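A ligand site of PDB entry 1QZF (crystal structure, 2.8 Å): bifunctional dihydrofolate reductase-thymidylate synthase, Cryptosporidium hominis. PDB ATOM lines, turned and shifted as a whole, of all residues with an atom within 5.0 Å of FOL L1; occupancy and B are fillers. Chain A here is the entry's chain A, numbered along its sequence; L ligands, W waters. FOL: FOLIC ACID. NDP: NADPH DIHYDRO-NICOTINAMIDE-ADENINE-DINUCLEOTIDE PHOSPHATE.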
ATOM      1  N   VAL A   9      -1.395   5.093  14.931  1.00  0.00           N
ATOM      2  CA  VAL A   9      -2.408   6.066  14.622  1.00  0.00           C
ATOM      3  C   VAL A   9      -1.907   7.323  15.278  1.00  0.00           C
ATOM      4  O   VAL A   9      -1.698   7.349  16.480  1.00  0.00           O
ATOM      5  CB  VAL A   9      -3.746   5.721  15.233  1.00  0.00           C
ATOM      6  CG1 VAL A   9      -4.786   6.721  14.776  1.00  0.00           C
ATOM      7  CG2 VAL A   9      -4.149   4.324  14.818  1.00  0.00           C
ATOM      8  N   VAL A  10      -1.692   8.368  14.488  1.00  0.00           N
ATOM      9  CA  VAL A  10      -1.193   9.598  15.054  1.00  0.00           C
ATOM     10  C   VAL A  10      -1.616  10.799  14.218  1.00  0.00           C
ATOM     11  O   VAL A  10      -1.948  10.681  13.041  1.00  0.00           O
ATOM     12  CB  VAL A  10       0.347   9.564  15.171  1.00  0.00           C
ATOM     13  CG1 VAL A  10       0.962   9.351  13.800  1.00  0.00           C
ATOM     14  CG2 VAL A  10       0.880  10.832  15.811  1.00  0.00           C
ATOM     15  N   ALA A  11      -1.603  11.949  14.872  1.00  0.00           N
ATOM     16  CA  ALA A  11      -1.945  13.207  14.244  1.00  0.00           C
ATOM     17  C   ALA A  11      -0.810  14.169  14.584  1.00  0.00           C
ATOM     18  O   ALA A  11      -0.597  14.471  15.757  1.00  0.00           O
ATOM     19  CB  ALA A  11      -3.263  13.709  14.785  1.00  0.00           C
ATOM     20  N   LEU A  25      -3.429  17.699  23.195  1.00  0.00           N
ATOM     21  CA  LEU A  25      -3.301  17.715  21.750  1.00  0.00           C
ATOM     22  C   LEU A  25      -3.211  19.201  21.466  1.00  0.00           C
ATOM     23  O   LEU A  25      -3.917  19.990  22.084  1.00  0.00           O
ATOM     24  CB  LEU A  25      -4.522  17.103  21.099  1.00  0.00           C
ATOM     25  CG  LEU A  25      -4.662  15.607  21.351  1.00  0.00           C
ATOM     26  CD1 LEU A  25      -6.010  15.122  20.871  1.00  0.00           C
ATOM     27  CD2 LEU A  25      -3.537  14.872  20.648  1.00  0.00           C
ATOM     28  N   SER A  30     -12.659  17.366  16.119  1.00  0.00           N
ATOM     29  CA  SER A  30     -13.470  16.208  16.459  1.00  0.00           C
ATOM     30  C   SER A  30     -13.473  15.127  15.375  1.00  0.00           C
ATOM     31  O   SER A  30     -13.470  13.940  15.684  1.00  0.00           O
ATOM     32  CB  SER A  30     -14.908  16.631  16.779  1.00  0.00           C
ATOM     33  OG  SER A  30     -15.468  17.428  15.756  1.00  0.00           O
ATOM     34  N   ASP A  32     -11.124  14.140  13.560  1.00  0.00           N
ATOM     35  CA  ASP A  32      -9.940  13.306  13.683  1.00  0.00           C
ATOM     36  C   ASP A  32     -10.061  12.360  14.870  1.00  0.00           C
ATOM     37  O   ASP A  32      -9.538  11.256  14.842  1.00  0.00           O
ATOM     38  CB  ASP A  32      -8.679  14.150  13.832  1.00  0.00           C
ATOM     39  CG  ASP A  32      -7.437  13.314  14.107  1.00  0.00           C
ATOM     40  OD1 ASP A  32      -7.210  12.335  13.365  1.00  0.00           O
ATOM     41  OD2 ASP A  32      -6.693  13.632  15.054  1.00  0.00           O
ATOM     42  N   LEU A  33     -10.729  12.811  15.928  1.00  0.00           N
ATOM     43  CA  LEU A  33     -10.912  11.939  17.074  1.00  0.00           C
ATOM     44  C   LEU A  33     -11.885  10.867  16.627  1.00  0.00           C
ATOM     45  O   LEU A  33     -11.738   9.697  16.951  1.00  0.00           O
ATOM     46  CB  LEU A  33     -11.489  12.707  18.248  1.00  0.00           C
ATOM     47  CG  LEU A  33     -10.490  13.520  19.064  1.00  0.00           C
ATOM     48  CD1 LEU A  33     -11.228  14.378  20.072  1.00  0.00           C
ATOM     49  CD2 LEU A  33      -9.525  12.598  19.766  1.00  0.00           C
ATOM     50  N   LYS A  34     -12.877  11.285  15.864  1.00  0.00           N
ATOM     51  CA  LYS A  34     -13.873  10.359  15.365  1.00  0.00           C
ATOM     52  C   LYS A  34     -13.161   9.331  14.469  1.00  0.00           C
ATOM     53  O   LYS A  34     -13.523   8.159  14.446  1.00  0.00           O
ATOM     54  CB  LYS A  34     -14.939  11.114  14.575  1.00  0.00           C
ATOM     55  CG  LYS A  34     -16.277  10.426  14.597  1.00  0.00           C
ATOM     56  CD  LYS A  34     -17.375  11.273  13.971  1.00  0.00           C
ATOM     57  CE  LYS A  34     -18.790  10.753  14.337  1.00  0.00           C
ATOM     58  NZ  LYS A  34     -19.096   9.331  13.915  1.00  0.00           N
ATOM     59  N   PHE A  35     -12.145   9.799  13.739  1.00  0.00           N
ATOM     60  CA  PHE A  35     -11.382   8.914  12.860  1.00  0.00           C
ATOM     61  C   PHE A  35     -10.653   7.907  13.717  1.00  0.00           C
ATOM     62  O   PHE A  35     -10.779   6.706  13.532  1.00  0.00           O
ATOM     63  CB  PHE A  35     -10.368   9.707  12.048  1.00  0.00           C
ATOM     64  CG  PHE A  35      -9.515   8.851  11.163  1.00  0.00           C
ATOM     65  CD1 PHE A  35     -10.079   8.119  10.126  1.00  0.00           C
ATOM     66  CD2 PHE A  35      -8.154   8.755  11.374  1.00  0.00           C
ATOM     67  CE1 PHE A  35      -9.300   7.287   9.324  1.00  0.00           C
ATOM     68  CE2 PHE A  35      -7.363   7.930  10.570  1.00  0.00           C
ATOM     69  CZ  PHE A  35      -7.944   7.204   9.546  1.00  0.00           C
ATOM     70  N   PHE A  36      -9.871   8.413  14.662  1.00  0.00           N
ATOM     71  CA  PHE A  36      -9.118   7.557  15.551  1.00  0.00           C
ATOM     72  C   PHE A  36     -10.040   6.484  16.100  1.00  0.00           C
ATOM     73  O   PHE A  36      -9.683   5.326  16.164  1.00  0.00           O
ATOM     74  CB  PHE A  36      -8.528   8.363  16.693  1.00  0.00           C
ATOM     75  CG  PHE A  36      -7.957   7.517  17.796  1.00  0.00           C
ATOM     76  CD1 PHE A  36      -8.783   6.924  18.731  1.00  0.00           C
ATOM     77  CD2 PHE A  36      -6.581   7.315  17.886  1.00  0.00           C
ATOM     78  CE1 PHE A  36      -8.266   6.135  19.731  1.00  0.00           C
ATOM     79  CE2 PHE A  36      -6.046   6.522  18.883  1.00  0.00           C
ATOM     80  CZ  PHE A  36      -6.892   5.934  19.811  1.00  0.00           C
ATOM     81  N   SER A  37     -11.237   6.894  16.501  1.00  0.00           N
ATOM     82  CA  SER A  37     -12.204   5.958  17.065  1.00  0.00           C
ATOM     83  C   SER A  37     -12.664   4.914  16.070  1.00  0.00           C
ATOM     84  O   SER A  37     -12.714   3.720  16.389  1.00  0.00           O
ATOM     85  CB  SER A  37     -13.401   6.719  17.607  1.00  0.00           C
ATOM     86  OG  SER A  37     -14.327   5.814  18.183  1.00  0.00           O
ATOM     87  N   THR A  40      -9.590   2.526  15.085  1.00  0.00           N
ATOM     88  CA  THR A  40      -9.141   1.636  16.150  1.00  0.00           C
ATOM     89  C   THR A  40     -10.210   0.677  16.641  1.00  0.00           C
ATOM     90  O   THR A  40      -9.933  -0.211  17.432  1.00  0.00           O
ATOM     91  CB  THR A  40      -8.629   2.414  17.368  1.00  0.00           C
ATOM     92  OG1 THR A  40      -9.700   3.167  17.929  1.00  0.00           O
ATOM     93  CG2 THR A  40      -7.505   3.334  16.960  1.00  0.00           C
ATOM     94  N   THR A  58       0.164   9.380  27.996  1.00  0.00           N
ATOM     95  CA  THR A  58      -1.014   9.465  27.144  1.00  0.00           C
ATOM     96  C   THR A  58      -2.210   8.921  27.919  1.00  0.00           C
ATOM     97  O   THR A  58      -3.316   9.437  27.823  1.00  0.00           O
ATOM     98  CB  THR A  58      -0.823   8.670  25.834  1.00  0.00           C
ATOM     99  OG1 THR A  58       0.164   9.316  25.032  1.00  0.00           O
ATOM    100  CG2 THR A  58      -2.124   8.605  25.049  1.00  0.00           C
ATOM    101  N   ILE A  62      -5.862  10.634  28.446  1.00  0.00           N
ATOM    102  CA  ILE A  62      -7.170  10.041  28.186  1.00  0.00           C
ATOM    103  C   ILE A  62      -8.060  10.168  29.425  1.00  0.00           C
ATOM    104  O   ILE A  62      -9.284  10.014  29.360  1.00  0.00           O
ATOM    105  CB  ILE A  62      -7.016   8.531  27.839  1.00  0.00           C
ATOM    106  CG1 ILE A  62      -6.386   8.376  26.463  1.00  0.00           C
ATOM    107  CG2 ILE A  62      -8.366   7.817  27.894  1.00  0.00           C
ATOM    108  CD1 ILE A  62      -7.385   8.324  25.330  1.00  0.00           C
ATOM    109  N   LEU A  67     -11.492   2.962  26.741  1.00  0.00           N
ATOM    110  CA  LEU A  67     -12.107   3.342  25.476  1.00  0.00           C
ATOM    111  C   LEU A  67     -13.044   2.185  25.127  1.00  0.00           C
ATOM    112  O   LEU A  67     -12.636   1.025  25.060  1.00  0.00           O
ATOM    113  CB  LEU A  67     -11.067   3.507  24.364  1.00  0.00           C
ATOM    114  CG  LEU A  67     -10.103   4.690  24.464  1.00  0.00           C
ATOM    115  CD1 LEU A  67      -9.040   4.585  23.407  1.00  0.00           C
ATOM    116  CD2 LEU A  67     -10.872   5.975  24.306  1.00  0.00           C
ATOM    117  N   ARG A  70     -12.813  -1.525  23.228  1.00  0.00           N
ATOM    118  CA  ARG A  70     -11.415  -1.825  23.042  1.00  0.00           C
ATOM    119  C   ARG A  70     -10.690  -2.168  24.338  1.00  0.00           C
ATOM    120  O   ARG A  70     -11.282  -2.199  25.417  1.00  0.00           O
ATOM    121  CB  ARG A  70     -10.736  -0.661  22.340  1.00  0.00           C
ATOM    122  CG  ARG A  70     -11.126  -0.538  20.881  1.00  0.00           C
ATOM    123  CD  ARG A  70     -11.076   0.895  20.443  1.00  0.00           C
ATOM    124  NE  ARG A  70     -12.167   1.656  21.058  1.00  0.00           N
ATOM    125  CZ  ARG A  70     -12.374   2.954  20.862  1.00  0.00           C
ATOM    126  NH1 ARG A  70     -11.562   3.644  20.069  1.00  0.00           N
ATOM    127  NH2 ARG A  70     -13.411   3.544  21.442  1.00  0.00           N
ATOM    128  N   CYS A 113      -1.048   3.556  19.904  1.00  0.00           N
ATOM    129  CA  CYS A 113      -1.742   4.814  20.048  1.00  0.00           C
ATOM    130  C   CYS A 113      -1.073   6.025  20.656  1.00  0.00           C
ATOM    131  O   CYS A 113      -1.754   6.912  21.145  1.00  0.00           O
ATOM    132  CB  CYS A 113      -3.055   4.574  20.773  1.00  0.00           C
ATOM    133  SG  CYS A 113      -4.119   3.403  19.939  1.00  0.00           S
ATOM    134  N   GLY A 114       0.243   6.090  20.657  1.00  0.00           N
ATOM    135  CA  GLY A 114       0.777   7.309  21.197  1.00  0.00           C
ATOM    136  C   GLY A 114       1.778   7.380  22.309  1.00  0.00           C
ATOM    137  O   GLY A 114       1.875   6.511  23.182  1.00  0.00           O
ATOM    138  N   TYR A 119       5.963   5.844  20.372  1.00  0.00           N
ATOM    139  CA  TYR A 119       6.005   5.818  18.913  1.00  0.00           C
ATOM    140  C   TYR A 119       7.428   5.485  18.491  1.00  0.00           C
ATOM    141  O   TYR A 119       7.673   4.514  17.777  1.00  0.00           O
ATOM    142  CB  TYR A 119       5.629   7.192  18.338  1.00  0.00           C
ATOM    143  CG  TYR A 119       4.145   7.521  18.345  1.00  0.00           C
ATOM    144  CD1 TYR A 119       3.202   6.569  17.950  1.00  0.00           C
ATOM    145  CD2 TYR A 119       3.704   8.791  18.668  1.00  0.00           C
ATOM    146  CE1 TYR A 119       1.860   6.887  17.881  1.00  0.00           C
ATOM    147  CE2 TYR A 119       2.365   9.119  18.599  1.00  0.00           C
ATOM    148  CZ  TYR A 119       1.443   8.172  18.200  1.00  0.00           C
ATOM    149  OH  TYR A 119       0.114   8.507  18.118  1.00  0.00           O
ATOM    150  N   THR A 134      -2.523  11.578  10.525  1.00  0.00           N
ATOM    151  CA  THR A 134      -3.389  12.701  10.226  1.00  0.00           C
ATOM    152  C   THR A 134      -2.474  13.911  10.242  1.00  0.00           C
ATOM    153  O   THR A 134      -1.839  14.210  11.249  1.00  0.00           O
ATOM    154  CB  THR A 134      -4.456  12.911  11.280  1.00  0.00           C
ATOM    155  OG1 THR A 134      -5.166  11.676  11.473  1.00  0.00           O
ATOM    156  CG2 THR A 134      -5.419  13.964  10.828  1.00  0.00           C
HETATM  157  N1  FOL L   1      -4.314   9.904  16.506  1.00  0.00           N
HETATM  158  C2  FOL L   1      -5.113  10.803  15.776  1.00  0.00           C
HETATM  159  NA2 FOL L   1      -5.081  10.810  14.450  1.00  0.00           N
HETATM  160  N3  FOL L   1      -5.951  11.673  16.476  1.00  0.00           N
HETATM  161  C4  FOL L   1      -5.997  11.643  17.876  1.00  0.00           C
HETATM  162  O4  FOL L   1      -6.633  12.507  18.480  1.00  0.00           O
HETATM  163  C4A FOL L   1      -5.223  10.738  18.591  1.00  0.00           C
HETATM  164  N5  FOL L   1      -5.229  10.740  19.993  1.00  0.00           N
HETATM  165  C6  FOL L   1      -4.339   9.943  20.735  1.00  0.00           C
HETATM  166  C7  FOL L   1      -3.462   9.104  20.027  1.00  0.00           C
HETATM  167  N8  FOL L   1      -3.485   9.069  18.631  1.00  0.00           N
HETATM  168  C8A FOL L   1      -4.369   9.886  17.898  1.00  0.00           C
HETATM  169  C9  FOL L   1      -4.458   9.733  22.103  1.00  0.00           C
HETATM  170  N10 FOL L   1      -5.415  10.114  22.919  1.00  0.00           N
HETATM  171  C11 FOL L   1      -9.383  10.315  22.614  1.00  0.00           C
HETATM  172  C12 FOL L   1      -8.643  10.035  21.466  1.00  0.00           C
HETATM  173  C13 FOL L   1      -7.266  10.210  21.474  1.00  0.00           C
HETATM  174  C14 FOL L   1      -6.603  10.646  22.624  1.00  0.00           C
HETATM  175  C15 FOL L   1      -7.353  10.988  23.741  1.00  0.00           C
HETATM  176  C16 FOL L   1      -8.739  10.816  23.735  1.00  0.00           C
HETATM  177  C   FOL L   1     -10.830   9.836  22.719  1.00  0.00           C
HETATM  178  O   FOL L   1     -11.573  10.272  23.608  1.00  0.00           O
HETATM  179  N   FOL L   1     -11.235   8.940  21.822  1.00  0.00           N
HETATM  180  CA  FOL L   1     -12.590   8.359  21.833  1.00  0.00           C
HETATM  181  CB  FOL L   1     -13.681   9.343  21.406  1.00  0.00           C
HETATM  182  CG  FOL L   1     -13.520   9.837  19.971  1.00  0.00           C
HETATM  183  CD  FOL L   1     -14.731  10.676  19.559  1.00  0.00           C
HETATM  184  OE1 FOL L   1     -14.641  11.922  19.658  1.00  0.00           O
HETATM  185  OE2 FOL L   1     -15.737  10.050  19.155  1.00  0.00           O
HETATM  186  CT  FOL L   1     -12.636   7.088  20.976  1.00  0.00           C
HETATM  187  O1  FOL L   1     -13.771   6.619  20.742  1.00  0.00           O
HETATM  188  O2  FOL L   1     -11.546   6.613  20.596  1.00  0.00           O
HETATM  189  PA  NDP L   2       4.017   8.936  26.308  1.00  0.00           P
HETATM  190  O1A NDP L   2       4.902   8.050  25.540  1.00  0.00           O
HETATM  191  O2A NDP L   2       2.534   8.840  26.297  1.00  0.00           O
HETATM  192  O5B NDP L   2       4.259   8.259  27.749  1.00  0.00           O
HETATM  193  C5B NDP L   2       5.555   8.156  28.337  1.00  0.00           C
HETATM  194  C4B NDP L   2       5.532   7.163  29.499  1.00  0.00           C
HETATM  195  O4B NDP L   2       5.288   5.786  29.065  1.00  0.00           O
HETATM  196  C3B NDP L   2       6.822   7.097  30.300  1.00  0.00           C
HETATM  197  O3B NDP L   2       6.838   8.118  31.303  1.00  0.00           O
HETATM  198  C2B NDP L   2       6.701   5.761  30.971  1.00  0.00           C
HETATM  199  O2B NDP L   2       5.801   5.860  32.071  1.00  0.00           O
HETATM  200  C1B NDP L   2       6.097   4.861  29.896  1.00  0.00           C
HETATM  201  N9A NDP L   2       7.200   4.328  29.058  1.00  0.00           N
HETATM  202  C8A NDP L   2       7.650   4.833  27.898  1.00  0.00           C
HETATM  203  N7A NDP L   2       8.658   4.085  27.459  1.00  0.00           N
HETATM  204  C5A NDP L   2       8.864   3.107  28.336  1.00  0.00           C
HETATM  205  C6A NDP L   2       9.760   2.051  28.394  1.00  0.00           C
HETATM  206  N6A NDP L   2      10.667   1.889  27.437  1.00  0.00           N
HETATM  207  N1A NDP L   2       9.699   1.183  29.446  1.00  0.00           N
HETATM  208  C2A NDP L   2       8.793   1.346  30.413  1.00  0.00           C
HETATM  209  N3A NDP L   2       7.922   2.365  30.372  1.00  0.00           N
HETATM  210  C4A NDP L   2       7.941   3.256  29.347  1.00  0.00           C
HETATM  211  O3  NDP L   2       4.593  10.398  26.783  1.00  0.00           O
HETATM  212  PN  NDP L   2       5.012  11.545  25.679  1.00  0.00           P
HETATM  213  O1N NDP L   2       6.031  10.742  24.956  1.00  0.00           O
HETATM  214  O2N NDP L   2       5.319  12.634  26.628  1.00  0.00           O
HETATM  215  O5D NDP L   2       3.520  11.516  25.007  1.00  0.00           O
HETATM  216  C5D NDP L   2       2.416  12.266  25.564  1.00  0.00           C
HETATM  217  C4D NDP L   2       2.239  13.597  24.803  1.00  0.00           C
HETATM  218  O4D NDP L   2       1.973  13.239  23.398  1.00  0.00           O
HETATM  219  C3D NDP L   2       0.979  14.336  25.256  1.00  0.00           C
HETATM  220  O3D NDP L   2       1.132  15.739  25.044  1.00  0.00           O
HETATM  221  C2D NDP L   2      -0.104  13.816  24.354  1.00  0.00           C
HETATM  222  O2D NDP L   2      -1.135  14.784  24.191  1.00  0.00           O
HETATM  223  C1D NDP L   2       0.616  13.643  23.045  1.00  0.00           C
HETATM  224  N1N NDP L   2      -0.038  12.694  22.122  1.00  0.00           N
HETATM  225  C2N NDP L   2      -0.393  13.131  20.820  1.00  0.00           C
HETATM  226  C3N NDP L   2      -0.920  12.214  19.914  1.00  0.00           C
HETATM  227  C7N NDP L   2      -1.286  12.654  18.482  1.00  0.00           C
HETATM  228  O7N NDP L   2      -1.718  11.843  17.668  1.00  0.00           O
HETATM  229  N7N NDP L   2      -1.099  13.941  18.217  1.00  0.00           N
HETATM  230  C4N NDP L   2      -1.092  10.869  20.300  1.00  0.00           C
HETATM  231  C5N NDP L   2      -0.749  10.435  21.583  1.00  0.00           C
HETATM  232  C6N NDP L   2      -0.223  11.343  22.500  1.00  0.00           C
HETATM  233  P2B NDP L   2       6.329   5.528  33.553  1.00  0.00           P
HETATM  234  O1X NDP L   2       4.999   5.668  34.462  1.00  0.00           O
HETATM  235  O2X NDP L   2       7.187   4.376  33.721  1.00  0.00           O
HETATM  236  O3X NDP L   2       7.015   6.795  33.861  1.00  0.00           O
HETATM  237  O   HOH W   1      -6.146  15.181  17.155  1.00  0.00           O
HETATM  238  O   HOH W   2      -4.263  12.637  23.616  1.00  0.00           O
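An oxygen (O1) of FOL L1 lies within hydrogen-bond range of the side-chain hydroxyl of Ser 37 (2.7 Å). The side-chain carboxylate (OD2) of Asp 32 sits at hydrogen-bond distance from a nitrogen (N3) of FOL L1 (2.5 Å). The backbone NH (N) of Ala 11 lies within hydrogen-bond range of an oxygen (O7N) of NDP L2, at 2.8 Å. N of Thr 58 is in hydrogen-bond range of O2A of NDP L2, 3.0 Å away. O of Val 9 lies close to N8 of FOL L1 (3.3 Å). The backbone carbonyl oxygen (O) of Val 10 is in hydrogen-bond range of a nitrogen (NA2) of FOL L1 (3.4 Å). NH1 of Arg 70 lies within salt-bridge range of O2 of FOL L1 (3.0 Å). An oxygen (O2A) of NDP L2 lies within hydrogen-bond range of the side-chain hydroxyl (OG1) of Thr 58. The side-chain hydroxyl (OG1) of Thr 134 lies within hydrogen-bond range of a nitrogen (NA2) of FOL L1 (3.1 Å). A nitrogen (N7N) of NDP L2 is in hydrogen-bond range of the backbone carbonyl oxygen (O) of Ala 11 (2.6 Å).
An oxygen (O7N) of NDP L2 sits close to a nitrogen (N8) of FOL L1 (3.4 Å).
The side-chain carboxylate (OD1) of Asp 32 is in hydrogen-bond range of the side-chain hydroxyl (OG1) of Thr 134. O of Val 10 sits at hydrogen-bond distance from N of Thr 134, at 2.7 Å. The side-chain hydroxyl (OG1) of Thr 40 is in hydrogen-bond range of the guanidinium group (NH1) of Arg 70 (2.9 Å). O of Val 9 sits at hydrogen-bond distance from OH of Tyr 119 (2.7 Å). O of Ser 37 lies within hydrogen-bond range of OG1 of Thr 40 (3.4 Å). The backbone carbonyl oxygen of Phe 36 is in hydrogen-bond range of the side-chain hydroxyl of Thr 40 (2.8 Å).
Residues that only touch FOL L1: Cys 113 (3.0 Å), Ile 62 (3.1 Å), Leu 33 (3.2 Å), Phe 36 (3.3 Å), Ala 11 (3.4 Å), Leu 25 (3.6 Å), Tyr 119 (3.7 Å), Leu 67 (3.8 Å) and Thr 58 (3.9 Å). 15 residues have an atom within 4 Å of FOL L1: Val 9, Val 10, Ala 11, Leu 25, Asp 32, Leu 33, Phe 36, Ser 37, Thr 58, Ile 62, Leu 67, Arg 70, Cys 113, Tyr 119 and Thr 134. Along chain A the residues within 4 Å of FOL L1 span positions 9 to 134.
Water W1 lies within hydrogen-bond range of the side-chain carboxylate (OD2) of Asp 32 (2.7 Å) and an oxygen (O4) of FOL L1 (3.0 Å).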
